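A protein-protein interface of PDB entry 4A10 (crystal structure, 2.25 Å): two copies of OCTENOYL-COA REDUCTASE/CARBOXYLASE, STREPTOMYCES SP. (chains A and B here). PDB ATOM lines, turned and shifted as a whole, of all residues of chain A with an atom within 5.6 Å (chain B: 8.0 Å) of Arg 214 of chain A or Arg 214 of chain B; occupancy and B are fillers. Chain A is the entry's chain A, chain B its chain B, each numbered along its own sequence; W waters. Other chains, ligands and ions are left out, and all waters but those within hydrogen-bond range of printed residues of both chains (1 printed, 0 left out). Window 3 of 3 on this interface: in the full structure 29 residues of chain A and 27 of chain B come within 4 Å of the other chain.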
ATOM      1  N   HIS A 152     -20.451  -3.004   6.788  1.00  0.00           N
ATOM      2  CA  HIS A 152     -20.285  -3.120   5.342  1.00  0.00           C
ATOM      3  C   HIS A 152     -20.528  -1.791   4.627  1.00  0.00           C
ATOM      4  O   HIS A 152     -20.469  -1.705   3.398  1.00  0.00           O
ATOM      5  CB  HIS A 152     -21.231  -4.199   4.803  1.00  0.00           C
ATOM      6  CG  HIS A 152     -20.929  -5.572   5.325  1.00  0.00           C
ATOM      7  ND1 HIS A 152     -20.531  -6.609   4.511  1.00  0.00           N
ATOM      8  CD2 HIS A 152     -20.951  -6.073   6.584  1.00  0.00           C
ATOM      9  CE1 HIS A 152     -20.331  -7.692   5.242  1.00  0.00           C
ATOM     10  NE2 HIS A 152     -20.574  -7.392   6.505  1.00  0.00           N
ATOM     11  N   GLY A 153     -20.845  -0.772   5.414  1.00  0.00           N
ATOM     12  CA  GLY A 153     -20.901   0.617   4.941  1.00  0.00           C
ATOM     13  C   GLY A 153     -19.734   1.428   5.459  1.00  0.00           C
ATOM     14  O   GLY A 153     -19.172   2.244   4.729  1.00  0.00           O
ATOM     15  N   ASP A 154     -19.358   1.197   6.720  1.00  0.00           N
ATOM     16  CA  ASP A 154     -18.175   1.835   7.340  1.00  0.00           C
ATOM     17  C   ASP A 154     -17.803   1.027   8.576  1.00  0.00           C
ATOM     18  O   ASP A 154     -18.559   0.980   9.546  1.00  0.00           O
ATOM     19  CB  ASP A 154     -18.494   3.297   7.702  1.00  0.00           C
ATOM     20  CG  ASP A 154     -17.298   4.073   8.319  1.00  0.00           C
ATOM     21  OD1 ASP A 154     -16.334   3.475   8.873  1.00  0.00           O
ATOM     22  OD2 ASP A 154     -17.379   5.322   8.291  1.00  0.00           O
ATOM     23  N   ARG A 208      -8.050   9.054   8.839  1.00  0.00           N
ATOM     24  CA  ARG A 208      -9.494   9.134   8.762  1.00  0.00           C
ATOM     25  C   ARG A 208      -9.921  10.579   8.925  1.00  0.00           C
ATOM     26  O   ARG A 208     -10.816  11.028   8.253  1.00  0.00           O
ATOM     27  CB  ARG A 208     -10.194   8.220   9.793  1.00  0.00           C
ATOM     28  CG  ARG A 208     -11.714   8.167   9.604  1.00  0.00           C
ATOM     29  CD  ARG A 208     -12.414   7.354  10.690  1.00  0.00           C
ATOM     30  NE  ARG A 208     -13.875   7.497  10.657  1.00  0.00           N
ATOM     31  CZ  ARG A 208     -14.716   6.686  10.006  1.00  0.00           C
ATOM     32  NH1 ARG A 208     -14.274   5.671   9.292  1.00  0.00           N
ATOM     33  NH2 ARG A 208     -16.021   6.890  10.080  1.00  0.00           N
ATOM     34  N   SER A 212      -9.204  10.616   4.433  1.00  0.00           N
ATOM     35  CA  SER A 212     -10.347   9.791   4.082  1.00  0.00           C
ATOM     36  C   SER A 212     -11.557  10.622   3.728  1.00  0.00           C
ATOM     37  O   SER A 212     -11.703  11.745   4.217  1.00  0.00           O
ATOM     38  CB  SER A 212     -10.718   8.926   5.276  1.00  0.00           C
ATOM     39  OG  SER A 212     -11.870   8.170   5.000  1.00  0.00           O
ATOM     40  N   ASP A 213     -12.443  10.044   2.915  1.00  0.00           N
ATOM     41  CA  ASP A 213     -13.737  10.653   2.672  1.00  0.00           C
ATOM     42  C   ASP A 213     -14.713  10.583   3.869  1.00  0.00           C
ATOM     43  O   ASP A 213     -15.789  11.164   3.802  1.00  0.00           O
ATOM     44  CB  ASP A 213     -14.374  10.138   1.363  1.00  0.00           C
ATOM     45  CG  ASP A 213     -14.744   8.642   1.400  1.00  0.00           C
ATOM     46  OD1 ASP A 213     -14.582   7.952   2.436  1.00  0.00           O
ATOM     47  OD2 ASP A 213     -15.234   8.154   0.350  1.00  0.00           O
ATOM     48  N   ARG A 214     -14.336   9.908   4.961  1.00  0.00           N
ATOM     49  CA  ARG A 214     -15.187   9.873   6.157  1.00  0.00           C
ATOM     50  C   ARG A 214     -14.815  10.969   7.171  1.00  0.00           C
ATOM     51  O   ARG A 214     -15.436  11.079   8.231  1.00  0.00           O
ATOM     52  CB  ARG A 214     -15.192   8.489   6.849  1.00  0.00           C
ATOM     53  CG  ARG A 214     -15.381   7.246   5.938  1.00  0.00           C
ATOM     54  CD  ARG A 214     -16.566   7.328   4.983  1.00  0.00           C
ATOM     55  NE  ARG A 214     -16.439   6.371   3.875  1.00  0.00           N
ATOM     56  CZ  ARG A 214     -16.906   5.114   3.895  1.00  0.00           C
ATOM     57  NH1 ARG A 214     -17.537   4.657   4.963  1.00  0.00           N
ATOM     58  NH2 ARG A 214     -16.736   4.307   2.848  1.00  0.00           N
ATOM     59  N   GLY A 215     -13.825  11.795   6.844  1.00  0.00           N
ATOM     60  CA  GLY A 215     -13.400  12.872   7.754  1.00  0.00           C
ATOM     61  C   GLY A 215     -13.496  14.217   7.068  1.00  0.00           C
ATOM     62  O   GLY A 215     -14.458  14.476   6.343  1.00  0.00           O
ATOM     63  N   ALA A 216     -12.471  15.046   7.264  1.00  0.00           N
ATOM     64  CA  ALA A 216     -12.403  16.390   6.696  1.00  0.00           C
ATOM     65  C   ALA A 216     -12.138  16.362   5.191  1.00  0.00           C
ATOM     66  O   ALA A 216     -12.588  17.252   4.448  1.00  0.00           O
ATOM     67  CB  ALA A 216     -11.327  17.209   7.416  1.00  0.00           C
ATOM     68  N   VAL A 358     -16.520  17.601  12.884  1.00  0.00           N
ATOM     69  CA  VAL A 358     -16.533  16.152  12.726  1.00  0.00           C
ATOM     70  C   VAL A 358     -15.829  15.499  13.918  1.00  0.00           C
ATOM     71  O   VAL A 358     -14.627  15.696  14.129  1.00  0.00           O
ATOM     72  CB  VAL A 358     -15.890  15.703  11.382  1.00  0.00           C
ATOM     73  CG1 VAL A 358     -15.875  14.153  11.260  1.00  0.00           C
ATOM     74  CG2 VAL A 358     -16.621  16.323  10.190  1.00  0.00           C
ATOM     75  N   SER A 360     -14.341  12.264  15.546  1.00  0.00           N
ATOM     76  CA  SER A 360     -13.786  11.056  14.971  1.00  0.00           C
ATOM     77  C   SER A 360     -12.733  10.440  15.851  1.00  0.00           C
ATOM     78  O   SER A 360     -12.030  11.137  16.579  1.00  0.00           O
ATOM     79  CB  SER A 360     -13.149  11.341  13.603  1.00  0.00           C
ATOM     80  OG  SER A 360     -12.840  10.127  12.916  1.00  0.00           O
ATOM     81  N   ASN A 364     -11.296   2.552   9.962  1.00  0.00           N
ATOM     82  CA  ASN A 364     -11.784   1.235   9.554  1.00  0.00           C
ATOM     83  C   ASN A 364     -10.702   0.445   8.784  1.00  0.00           C
ATOM     84  O   ASN A 364      -9.673   1.004   8.402  1.00  0.00           O
ATOM     85  CB  ASN A 364     -13.130   1.348   8.809  1.00  0.00           C
ATOM     86  CG  ASN A 364     -13.011   2.027   7.455  1.00  0.00           C
ATOM     87  OD1 ASN A 364     -12.010   1.886   6.764  1.00  0.00           O
ATOM     88  ND2 ASN A 364     -14.060   2.753   7.063  1.00  0.00           N
ATOM     89  N   GLU A 366     -10.455  -0.533   5.768  1.00  0.00           N
ATOM     90  CA  GLU A 366     -10.125   0.087   4.484  1.00  0.00           C
ATOM     91  C   GLU A 366      -9.173   1.280   4.614  1.00  0.00           C
ATOM     92  O   GLU A 366      -8.205   1.381   3.874  1.00  0.00           O
ATOM     93  CB  GLU A 366     -11.377   0.504   3.694  1.00  0.00           C
ATOM     94  CG  GLU A 366     -10.987   1.366   2.509  1.00  0.00           C
ATOM     95  CD  GLU A 366     -11.698   1.030   1.252  1.00  0.00           C
ATOM     96  OE1 GLU A 366     -12.890   1.403   1.149  1.00  0.00           O
ATOM     97  OE2 GLU A 366     -11.063   0.419   0.349  1.00  0.00           O
ATOM     98  N   GLU A 367      -9.458   2.169   5.555  1.00  0.00           N
ATOM     99  CA  GLU A 367      -8.566   3.297   5.850  1.00  0.00           C
ATOM    100  C   GLU A 367      -7.191   2.842   6.344  1.00  0.00           C
ATOM    101  O   GLU A 367      -6.165   3.440   5.991  1.00  0.00           O
ATOM    102  CB  GLU A 367      -9.232   4.242   6.852  1.00  0.00           C
ATOM    103  CG  GLU A 367     -10.473   4.898   6.268  1.00  0.00           C
ATOM    104  CD  GLU A 367     -11.415   5.539   7.287  1.00  0.00           C
ATOM    105  OE1 GLU A 367     -11.575   4.997   8.407  1.00  0.00           O
ATOM    106  OE2 GLU A 367     -12.005   6.604   6.951  1.00  0.00           O
ATOM    107  N   ALA B 150     -11.314  -3.585   1.644  1.00  0.00           N
ATOM    108  CA  ALA B 150     -12.368  -2.873   0.876  1.00  0.00           C
ATOM    109  C   ALA B 150     -13.814  -3.116   1.373  1.00  0.00           C
ATOM    110  O   ALA B 150     -14.644  -2.209   1.358  1.00  0.00           O
ATOM    111  CB  ALA B 150     -12.241  -3.167  -0.612  1.00  0.00           C
ATOM    112  N   THR B 151     -14.102  -4.336   1.815  1.00  0.00           N
ATOM    113  CA  THR B 151     -15.400  -4.676   2.417  1.00  0.00           C
ATOM    114  C   THR B 151     -15.848  -3.697   3.524  1.00  0.00           C
ATOM    115  O   THR B 151     -17.051  -3.408   3.656  1.00  0.00           O
ATOM    116  CB  THR B 151     -15.401  -6.135   2.921  1.00  0.00           C
ATOM    117  OG1 THR B 151     -15.141  -7.015   1.816  1.00  0.00           O
ATOM    118  CG2 THR B 151     -16.749  -6.520   3.557  1.00  0.00           C
ATOM    119  N   HIS B 152     -14.881  -3.193   4.300  1.00  0.00           N
ATOM    120  CA  HIS B 152     -15.131  -2.261   5.414  1.00  0.00           C
ATOM    121  C   HIS B 152     -15.304  -0.791   5.006  1.00  0.00           C
ATOM    122  O   HIS B 152     -15.446   0.107   5.864  1.00  0.00           O
ATOM    123  CB  HIS B 152     -14.009  -2.377   6.438  1.00  0.00           C
ATOM    124  CG  HIS B 152     -13.899  -3.739   7.048  1.00  0.00           C
ATOM    125  ND1 HIS B 152     -14.337  -4.021   8.321  1.00  0.00           N
ATOM    126  CD2 HIS B 152     -13.422  -4.903   6.547  1.00  0.00           C
ATOM    127  CE1 HIS B 152     -14.109  -5.295   8.592  1.00  0.00           C
ATOM    128  NE2 HIS B 152     -13.560  -5.855   7.531  1.00  0.00           N
ATOM    129  N   GLY B 153     -15.233  -0.543   3.706  1.00  0.00           N
ATOM    130  CA  GLY B 153     -15.560   0.754   3.161  1.00  0.00           C
ATOM    131  C   GLY B 153     -16.847   0.654   2.374  1.00  0.00           C
ATOM    132  O   GLY B 153     -17.608   1.612   2.328  1.00  0.00           O
ATOM    133  N   ASP B 154     -17.084  -0.522   1.772  1.00  0.00           N
ATOM    134  CA  ASP B 154     -18.257  -0.806   0.931  1.00  0.00           C
ATOM    135  C   ASP B 154     -18.287  -2.305   0.622  1.00  0.00           C
ATOM    136  O   ASP B 154     -17.457  -2.820  -0.116  1.00  0.00           O
ATOM    137  CB  ASP B 154     -18.226   0.008  -0.375  1.00  0.00           C
ATOM    138  CG  ASP B 154     -19.530  -0.134  -1.253  1.00  0.00           C
ATOM    139  OD1 ASP B 154     -20.307  -1.107  -1.185  1.00  0.00           O
ATOM    140  OD2 ASP B 154     -19.758   0.785  -2.053  1.00  0.00           O
ATOM    141  N   GLY B 155     -19.264  -2.993   1.191  1.00  0.00           N
ATOM    142  CA  GLY B 155     -19.421  -4.420   0.976  1.00  0.00           C
ATOM    143  C   GLY B 155     -19.352  -4.873  -0.471  1.00  0.00           C
ATOM    144  O   GLY B 155     -18.854  -5.957  -0.737  1.00  0.00           O
ATOM    145  N   MET B 156     -19.820  -4.041  -1.406  1.00  0.00           N
ATOM    146  CA  MET B 156     -19.814  -4.409  -2.832  1.00  0.00           C
ATOM    147  C   MET B 156     -18.474  -4.268  -3.574  1.00  0.00           C
ATOM    148  O   MET B 156     -18.342  -4.758  -4.696  1.00  0.00           O
ATOM    149  CB  MET B 156     -20.920  -3.669  -3.593  1.00  0.00           C
ATOM    150  CG  MET B 156     -22.324  -4.130  -3.238  1.00  0.00           C
ATOM    151  SD  MET B 156     -22.669  -5.870  -3.615  1.00  0.00           S
ATOM    152  CE  MET B 156     -22.401  -5.928  -5.390  1.00  0.00           C
ATOM    153  N   LEU B 157     -17.482  -3.646  -2.930  1.00  0.00           N
ATOM    154  CA  LEU B 157     -16.238  -3.246  -3.601  1.00  0.00           C
ATOM    155  C   LEU B 157     -15.090  -4.230  -3.481  1.00  0.00           C
ATOM    156  O   LEU B 157     -14.127  -4.142  -4.243  1.00  0.00           O
ATOM    157  CB  LEU B 157     -15.776  -1.863  -3.104  1.00  0.00           C
ATOM    158  CG  LEU B 157     -16.227  -0.654  -3.909  1.00  0.00           C
ATOM    159  CD1 LEU B 157     -17.664  -0.792  -4.423  1.00  0.00           C
ATOM    160  CD2 LEU B 157     -16.030   0.656  -3.120  1.00  0.00           C
ATOM    161  N   TYR B 207     -32.404   0.023  -4.627  1.00  0.00           N
ATOM    162  CA  TYR B 207     -32.079   0.879  -3.498  1.00  0.00           C
ATOM    163  C   TYR B 207     -30.670   1.467  -3.657  1.00  0.00           C
ATOM    164  O   TYR B 207     -30.449   2.689  -3.479  1.00  0.00           O
ATOM    165  CB  TYR B 207     -32.225   0.122  -2.173  1.00  0.00           C
ATOM    166  CG  TYR B 207     -31.942   0.984  -0.982  1.00  0.00           C
ATOM    167  CD1 TYR B 207     -30.631   1.267  -0.604  1.00  0.00           C
ATOM    168  CD2 TYR B 207     -32.987   1.546  -0.238  1.00  0.00           C
ATOM    169  CE1 TYR B 207     -30.356   2.073   0.482  1.00  0.00           C
ATOM    170  CE2 TYR B 207     -32.728   2.354   0.843  1.00  0.00           C
ATOM    171  CZ  TYR B 207     -31.409   2.624   1.198  1.00  0.00           C
ATOM    172  OH  TYR B 207     -31.133   3.446   2.278  1.00  0.00           O
ATOM    173  N   ARG B 208     -29.717   0.600  -3.988  1.00  0.00           N
ATOM    174  CA  ARG B 208     -28.366   1.066  -4.191  1.00  0.00           C
ATOM    175  C   ARG B 208     -28.331   2.082  -5.328  1.00  0.00           C
ATOM    176  O   ARG B 208     -27.769   3.148  -5.182  1.00  0.00           O
ATOM    177  CB  ARG B 208     -27.362  -0.068  -4.419  1.00  0.00           C
ATOM    178  CG  ARG B 208     -25.918   0.447  -4.414  1.00  0.00           C
ATOM    179  CD  ARG B 208     -24.876  -0.641  -4.685  1.00  0.00           C
ATOM    180  NE  ARG B 208     -23.525  -0.095  -4.904  1.00  0.00           N
ATOM    181  CZ  ARG B 208     -22.563  -0.043  -3.975  1.00  0.00           C
ATOM    182  NH1 ARG B 208     -22.786  -0.498  -2.744  1.00  0.00           N
ATOM    183  NH2 ARG B 208     -21.357   0.441  -4.280  1.00  0.00           N
ATOM    184  N   MET B 209     -28.981   1.764  -6.435  1.00  0.00           N
ATOM    185  CA  MET B 209     -28.991   2.662  -7.587  1.00  0.00           C
ATOM    186  C   MET B 209     -29.582   4.042  -7.295  1.00  0.00           C
ATOM    187  O   MET B 209     -29.064   5.024  -7.786  1.00  0.00           O
ATOM    188  CB  MET B 209     -29.689   2.008  -8.784  1.00  0.00           C
ATOM    189  CG  MET B 209     -28.859   0.881  -9.394  1.00  0.00           C
ATOM    190  SD  MET B 209     -29.876  -0.161 -10.457  1.00  0.00           S
ATOM    191  CE  MET B 209     -29.696   0.682 -12.046  1.00  0.00           C
ATOM    192  N   LEU B 210     -30.622   4.100  -6.463  1.00  0.00           N
ATOM    193  CA  LEU B 210     -31.465   5.293  -6.342  1.00  0.00           C
ATOM    194  C   LEU B 210     -31.434   6.042  -5.023  1.00  0.00           C
ATOM    195  O   LEU B 210     -31.427   7.266  -5.014  1.00  0.00           O
ATOM    196  CB  LEU B 210     -32.919   4.936  -6.661  1.00  0.00           C
ATOM    197  CG  LEU B 210     -33.250   4.742  -8.130  1.00  0.00           C
ATOM    198  CD1 LEU B 210     -34.661   4.213  -8.268  1.00  0.00           C
ATOM    199  CD2 LEU B 210     -33.079   6.061  -8.881  1.00  0.00           C
ATOM    200  N   VAL B 211     -31.433   5.312  -3.913  1.00  0.00           N
ATOM    201  CA  VAL B 211     -31.582   5.901  -2.583  1.00  0.00           C
ATOM    202  C   VAL B 211     -30.245   6.107  -1.875  1.00  0.00           C
ATOM    203  O   VAL B 211     -29.976   7.171  -1.297  1.00  0.00           O
ATOM    204  CB  VAL B 211     -32.472   4.991  -1.683  1.00  0.00           C
ATOM    205  CG1 VAL B 211     -32.809   5.680  -0.358  1.00  0.00           C
ATOM    206  CG2 VAL B 211     -33.741   4.602  -2.420  1.00  0.00           C
ATOM    207  N   SER B 212     -29.423   5.064  -1.903  1.00  0.00           N
ATOM    208  CA  SER B 212     -28.153   5.033  -1.183  1.00  0.00           C
ATOM    209  C   SER B 212     -27.171   6.145  -1.595  1.00  0.00           C
ATOM    210  O   SER B 212     -27.244   6.654  -2.712  1.00  0.00           O
ATOM    211  CB  SER B 212     -27.481   3.695  -1.421  1.00  0.00           C
ATOM    212  OG  SER B 212     -26.172   3.724  -0.903  1.00  0.00           O
ATOM    213  N   ASP B 213     -26.231   6.484  -0.702  1.00  0.00           N
ATOM    214  CA  ASP B 213     -25.156   7.399  -1.085  1.00  0.00           C
ATOM    215  C   ASP B 213     -24.118   6.804  -2.076  1.00  0.00           C
ATOM    216  O   ASP B 213     -23.257   7.510  -2.556  1.00  0.00           O
ATOM    217  CB  ASP B 213     -24.505   8.101   0.117  1.00  0.00           C
ATOM    218  CG  ASP B 213     -23.744   7.150   1.063  1.00  0.00           C
ATOM    219  OD1 ASP B 213     -23.675   5.905   0.848  1.00  0.00           O
ATOM    220  OD2 ASP B 213     -23.197   7.691   2.061  1.00  0.00           O
ATOM    221  N   ARG B 214     -24.214   5.514  -2.391  1.00  0.00           N
ATOM    222  CA  ARG B 214     -23.238   4.913  -3.291  1.00  0.00           C
ATOM    223  C   ARG B 214     -23.795   4.853  -4.704  1.00  0.00           C
ATOM    224  O   ARG B 214     -23.179   4.286  -5.596  1.00  0.00           O
ATOM    225  CB  ARG B 214     -22.794   3.525  -2.805  1.00  0.00           C
ATOM    226  CG  ARG B 214     -22.467   3.434  -1.309  1.00  0.00           C
ATOM    227  CD  ARG B 214     -21.352   4.358  -0.864  1.00  0.00           C
ATOM    228  NE  ARG B 214     -21.249   4.448   0.604  1.00  0.00           N
ATOM    229  CZ  ARG B 214     -20.627   3.553   1.369  1.00  0.00           C
ATOM    230  NH1 ARG B 214     -20.068   2.491   0.814  1.00  0.00           N
ATOM    231  NH2 ARG B 214     -20.564   3.706   2.694  1.00  0.00           N
ATOM    232  N   GLY B 215     -24.956   5.463  -4.904  1.00  0.00           N
ATOM    233  CA  GLY B 215     -25.585   5.471  -6.230  1.00  0.00           C
ATOM    234  C   GLY B 215     -25.929   6.879  -6.650  1.00  0.00           C
ATOM    235  O   GLY B 215     -25.201   7.818  -6.333  1.00  0.00           O
ATOM    236  N   ALA B 216     -27.064   7.014  -7.328  1.00  0.00           N
ATOM    237  CA  ALA B 216     -27.583   8.314  -7.770  1.00  0.00           C
ATOM    238  C   ALA B 216     -27.969   9.221  -6.610  1.00  0.00           C
ATOM    239  O   ALA B 216     -27.917  10.456  -6.741  1.00  0.00           O
ATOM    240  CB  ALA B 216     -28.775   8.125  -8.702  1.00  0.00           C
ATOM    241  N   GLN B 217     -28.363   8.608  -5.490  1.00  0.00           N
ATOM    242  CA  GLN B 217     -28.826   9.324  -4.293  1.00  0.00           C
ATOM    243  C   GLN B 217     -29.859  10.414  -4.596  1.00  0.00           C
ATOM    244  O   GLN B 217     -29.553  11.607  -4.535  1.00  0.00           O
ATOM    245  CB  GLN B 217     -27.638   9.919  -3.517  1.00  0.00           C
ATOM    246  CG  GLN B 217     -27.938  10.177  -2.043  1.00  0.00           C
ATOM    247  CD  GLN B 217     -26.720  10.719  -1.265  1.00  0.00           C
ATOM    248  OE1 GLN B 217     -25.637  10.904  -1.821  1.00  0.00           O
ATOM    249  NE2 GLN B 217     -26.913  10.990   0.023  1.00  0.00           N
ATOM    250  N   VAL B 333     -27.915   5.941 -14.121  1.00  0.00           N
ATOM    251  CA  VAL B 333     -27.479   4.781 -13.355  1.00  0.00           C
ATOM    252  C   VAL B 333     -27.921   3.529 -14.117  1.00  0.00           C
ATOM    253  O   VAL B 333     -29.054   3.438 -14.586  1.00  0.00           O
ATOM    254  CB  VAL B 333     -27.975   4.828 -11.888  1.00  0.00           C
ATOM    255  CG1 VAL B 333     -27.514   3.605 -11.098  1.00  0.00           C
ATOM    256  CG2 VAL B 333     -27.400   6.041 -11.203  1.00  0.00           C
ATOM    257  N   VAL B 358     -23.454   6.126 -13.531  1.00  0.00           N
ATOM    258  CA  VAL B 358     -23.078   5.279 -12.430  1.00  0.00           C
ATOM    259  C   VAL B 358     -23.444   3.821 -12.743  1.00  0.00           C
ATOM    260  O   VAL B 358     -24.614   3.473 -12.904  1.00  0.00           O
ATOM    261  CB  VAL B 358     -23.617   5.800 -11.067  1.00  0.00           C
ATOM    262  CG1 VAL B 358     -23.099   4.939  -9.937  1.00  0.00           C
ATOM    263  CG2 VAL B 358     -23.172   7.274 -10.837  1.00  0.00           C
ATOM    264  N   GLY B 359     -22.405   2.996 -12.879  1.00  0.00           N
ATOM    265  CA  GLY B 359     -22.585   1.573 -13.148  1.00  0.00           C
ATOM    266  C   GLY B 359     -22.763   0.899 -11.807  1.00  0.00           C
ATOM    267  O   GLY B 359     -21.923   1.046 -10.919  1.00  0.00           O
ATOM    268  N   SER B 360     -23.865   0.183 -11.643  1.00  0.00           N
ATOM    269  CA  SER B 360     -24.180  -0.402 -10.350  1.00  0.00           C
ATOM    270  C   SER B 360     -24.822  -1.781 -10.448  1.00  0.00           C
ATOM    271  O   SER B 360     -25.536  -2.075 -11.403  1.00  0.00           O
ATOM    272  CB  SER B 360     -25.103   0.531  -9.570  1.00  0.00           C
ATOM    273  OG  SER B 360     -25.157   0.132  -8.207  1.00  0.00           O
ATOM    274  N   ASN B 364     -24.763  -3.811  -0.680  1.00  0.00           N
ATOM    275  CA  ASN B 364     -24.040  -4.364   0.454  1.00  0.00           C
ATOM    276  C   ASN B 364     -24.975  -4.595   1.644  1.00  0.00           C
ATOM    277  O   ASN B 364     -26.125  -4.179   1.618  1.00  0.00           O
ATOM    278  CB  ASN B 364     -22.830  -3.478   0.815  1.00  0.00           C
ATOM    279  CG  ASN B 364     -23.233  -2.072   1.273  1.00  0.00           C
ATOM    280  OD1 ASN B 364     -24.234  -1.891   1.968  1.00  0.00           O
ATOM    281  ND2 ASN B 364     -22.425  -1.071   0.892  1.00  0.00           N
ATOM    282  N   GLU B 366     -25.315  -3.291   4.579  1.00  0.00           N
ATOM    283  CA  GLU B 366     -25.936  -2.086   5.145  1.00  0.00           C
ATOM    284  C   GLU B 366     -27.128  -1.595   4.328  1.00  0.00           C
ATOM    285  O   GLU B 366     -28.196  -1.315   4.898  1.00  0.00           O
ATOM    286  CB  GLU B 366     -24.909  -0.954   5.300  1.00  0.00           C
ATOM    287  CG  GLU B 366     -25.506   0.350   5.839  1.00  0.00           C
ATOM    288  CD  GLU B 366     -24.624   1.560   5.577  1.00  0.00           C
ATOM    289  OE1 GLU B 366     -24.220   1.780   4.407  1.00  0.00           O
ATOM    290  OE2 GLU B 366     -24.339   2.296   6.541  1.00  0.00           O
ATOM    291  N   GLU B 367     -26.943  -1.497   3.010  1.00  0.00           N
ATOM    292  CA  GLU B 367     -28.034  -1.141   2.092  1.00  0.00           C
ATOM    293  C   GLU B 367     -29.226  -2.127   2.151  1.00  0.00           C
ATOM    294  O   GLU B 367     -30.376  -1.729   2.028  1.00  0.00           O
ATOM    295  CB  GLU B 367     -27.510  -1.016   0.647  1.00  0.00           C
ATOM    296  CG  GLU B 367     -26.583   0.199   0.435  1.00  0.00           C
ATOM    297  CD  GLU B 367     -25.676   0.112  -0.813  1.00  0.00           C
ATOM    298  OE1 GLU B 367     -25.281  -1.005  -1.233  1.00  0.00           O
ATOM    299  OE2 GLU B 367     -25.355   1.186  -1.382  1.00  0.00           O
HETATM  300  O   HOH W   1     -14.370  -0.027  -0.351  1.00  0.00           O
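Of chain B, only Gly 153 and Arg 214 come within 4 Å of Arg 214 of chain A.
No residue of chain B comes within 4 Å of Gly 215 of chain A.
Val 358 of chain A touches none of the printed residues of chain B.
Printed residues of chain A within 4 Å of Asp 154 of chain B: His 152.
Of the printed residues of chain A, Gly 155 of chain B touches His 152.
Arg 214 of chain B touches just these residues of chain A: Gly 153 (2.9 Å) and Arg 214 (3.9 Å).
The nearest residue of chain B that does not touch Arg 214 of chain A is Asp 154 of chain B (5.0 Å).
Printed residues of chain B that touch a printed residue of chain A: Ala 150, Thr 151, His 152, Gly 153, Asp 154, Gly 155, Arg 214, Asn 364 and Glu 366.
Hydrophobic or aromatic side chains of chain B within 4 Å of the printed part of chain A: Ala 150.
Of the 14 printed residues of chain A, 6 touch a printed residue of chain B.
Printed residues of chain A that touch a printed residue of chain B: His 152, Gly 153, Asp 154, Arg 214, Asn 364 and Glu 366.
Hydrophobic or aromatic side chains of chain A that line the printed part of chain B: His 152.
N of Gly 155 of chain B is in hydrogen-bond range of O of His 152 of chain A (2.8 Å).
ND2 of Asn 364 of chain B sits at hydrogen-bond distance from O of His 152 of chain A (3.2 Å).
O of Gly 153 of chain A is in hydrogen-bond range of NH2 of Arg 214 of chain B (2.9 Å).
The guanidinium group (NH2) of Arg 214 of chain A is in hydrogen-bond range of the backbone carbonyl oxygen (O) of Gly 153 of chain B, 2.9 Å away.
O of His 152 of chain B sits at hydrogen-bond distance from ND2 of Asn 364 of chain A (3.2 Å).
The backbone carbonyl oxygen of Gly 153 of chain A lies close to the backbone carbonyl oxygen of Gly 153 of chain B (2.9 Å).
Among the printed residues, merely in contact across the chains: Glu 366 of chain A with Gly 153 of chain B, His 152 of chain A with Asp 154 of chain B, Asp 154 of chain A with His 152 of chain B, Gly 153 of chain A with Glu 366 of chain B, Glu 366 of chain A with Ala 150 of chain B, His 152 of chain A with Thr 151 of chain B and Arg 214 of chain A with Arg 214 of chain B.
Water W1 lies within hydrogen-bond range of the side-chain carboxylate of Glu 366 of chain A, the backbone carbonyl oxygen of Ala 150 of chain B and the backbone NH of Asp 154 of chain B.
O of Gly 153 of chain A sits at hydrogen-bond distance from NH1 of Arg 214 of chain A, at 2.9 Å.
OG of Ser 212 of chain A is in hydrogen-bond range of N of Arg 214 of chain A, 3.0 Å away.
The backbone NH (N) of Glu 366 of chain A is in hydrogen-bond range of the side-chain amide oxygen (OD1) of Asn 364 of chain A (3.0 Å).
O of Gly 153 of chain B lies within hydrogen-bond range of NH1 of Arg 214 of chain B (3.0 Å).
OD2 of Asp 154 of chain B is in salt-bridge range of NH2 of Arg 208 of chain B, 2.8 Å away.
The backbone NH (N) of Glu 366 of chain B sits at hydrogen-bond distance from the side-chain amide oxygen (OD1) of Asn 364 of chain B (3.2 Å).
His 152 of chain A touches Asp 154 of chain B, and with the chains exchanged Asp 154 of chain A touches His 152 of chain B.
His 152 of chain A touches Asn 364 of chain B, and with the chains exchanged Asn 364 of chain A touches His 152 of chain B.
Gly 153 of chain A touches Arg 214 of chain B, and with the chains exchanged Arg 214 of chain A touches Gly 153 of chain B.
Arg 214 of chain A touches its own counterpart, Arg 214 of chain B.
Of the 13 pairs that touch across the chains among the printed residues, 10 have their exchanged pair printed and touching as well.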
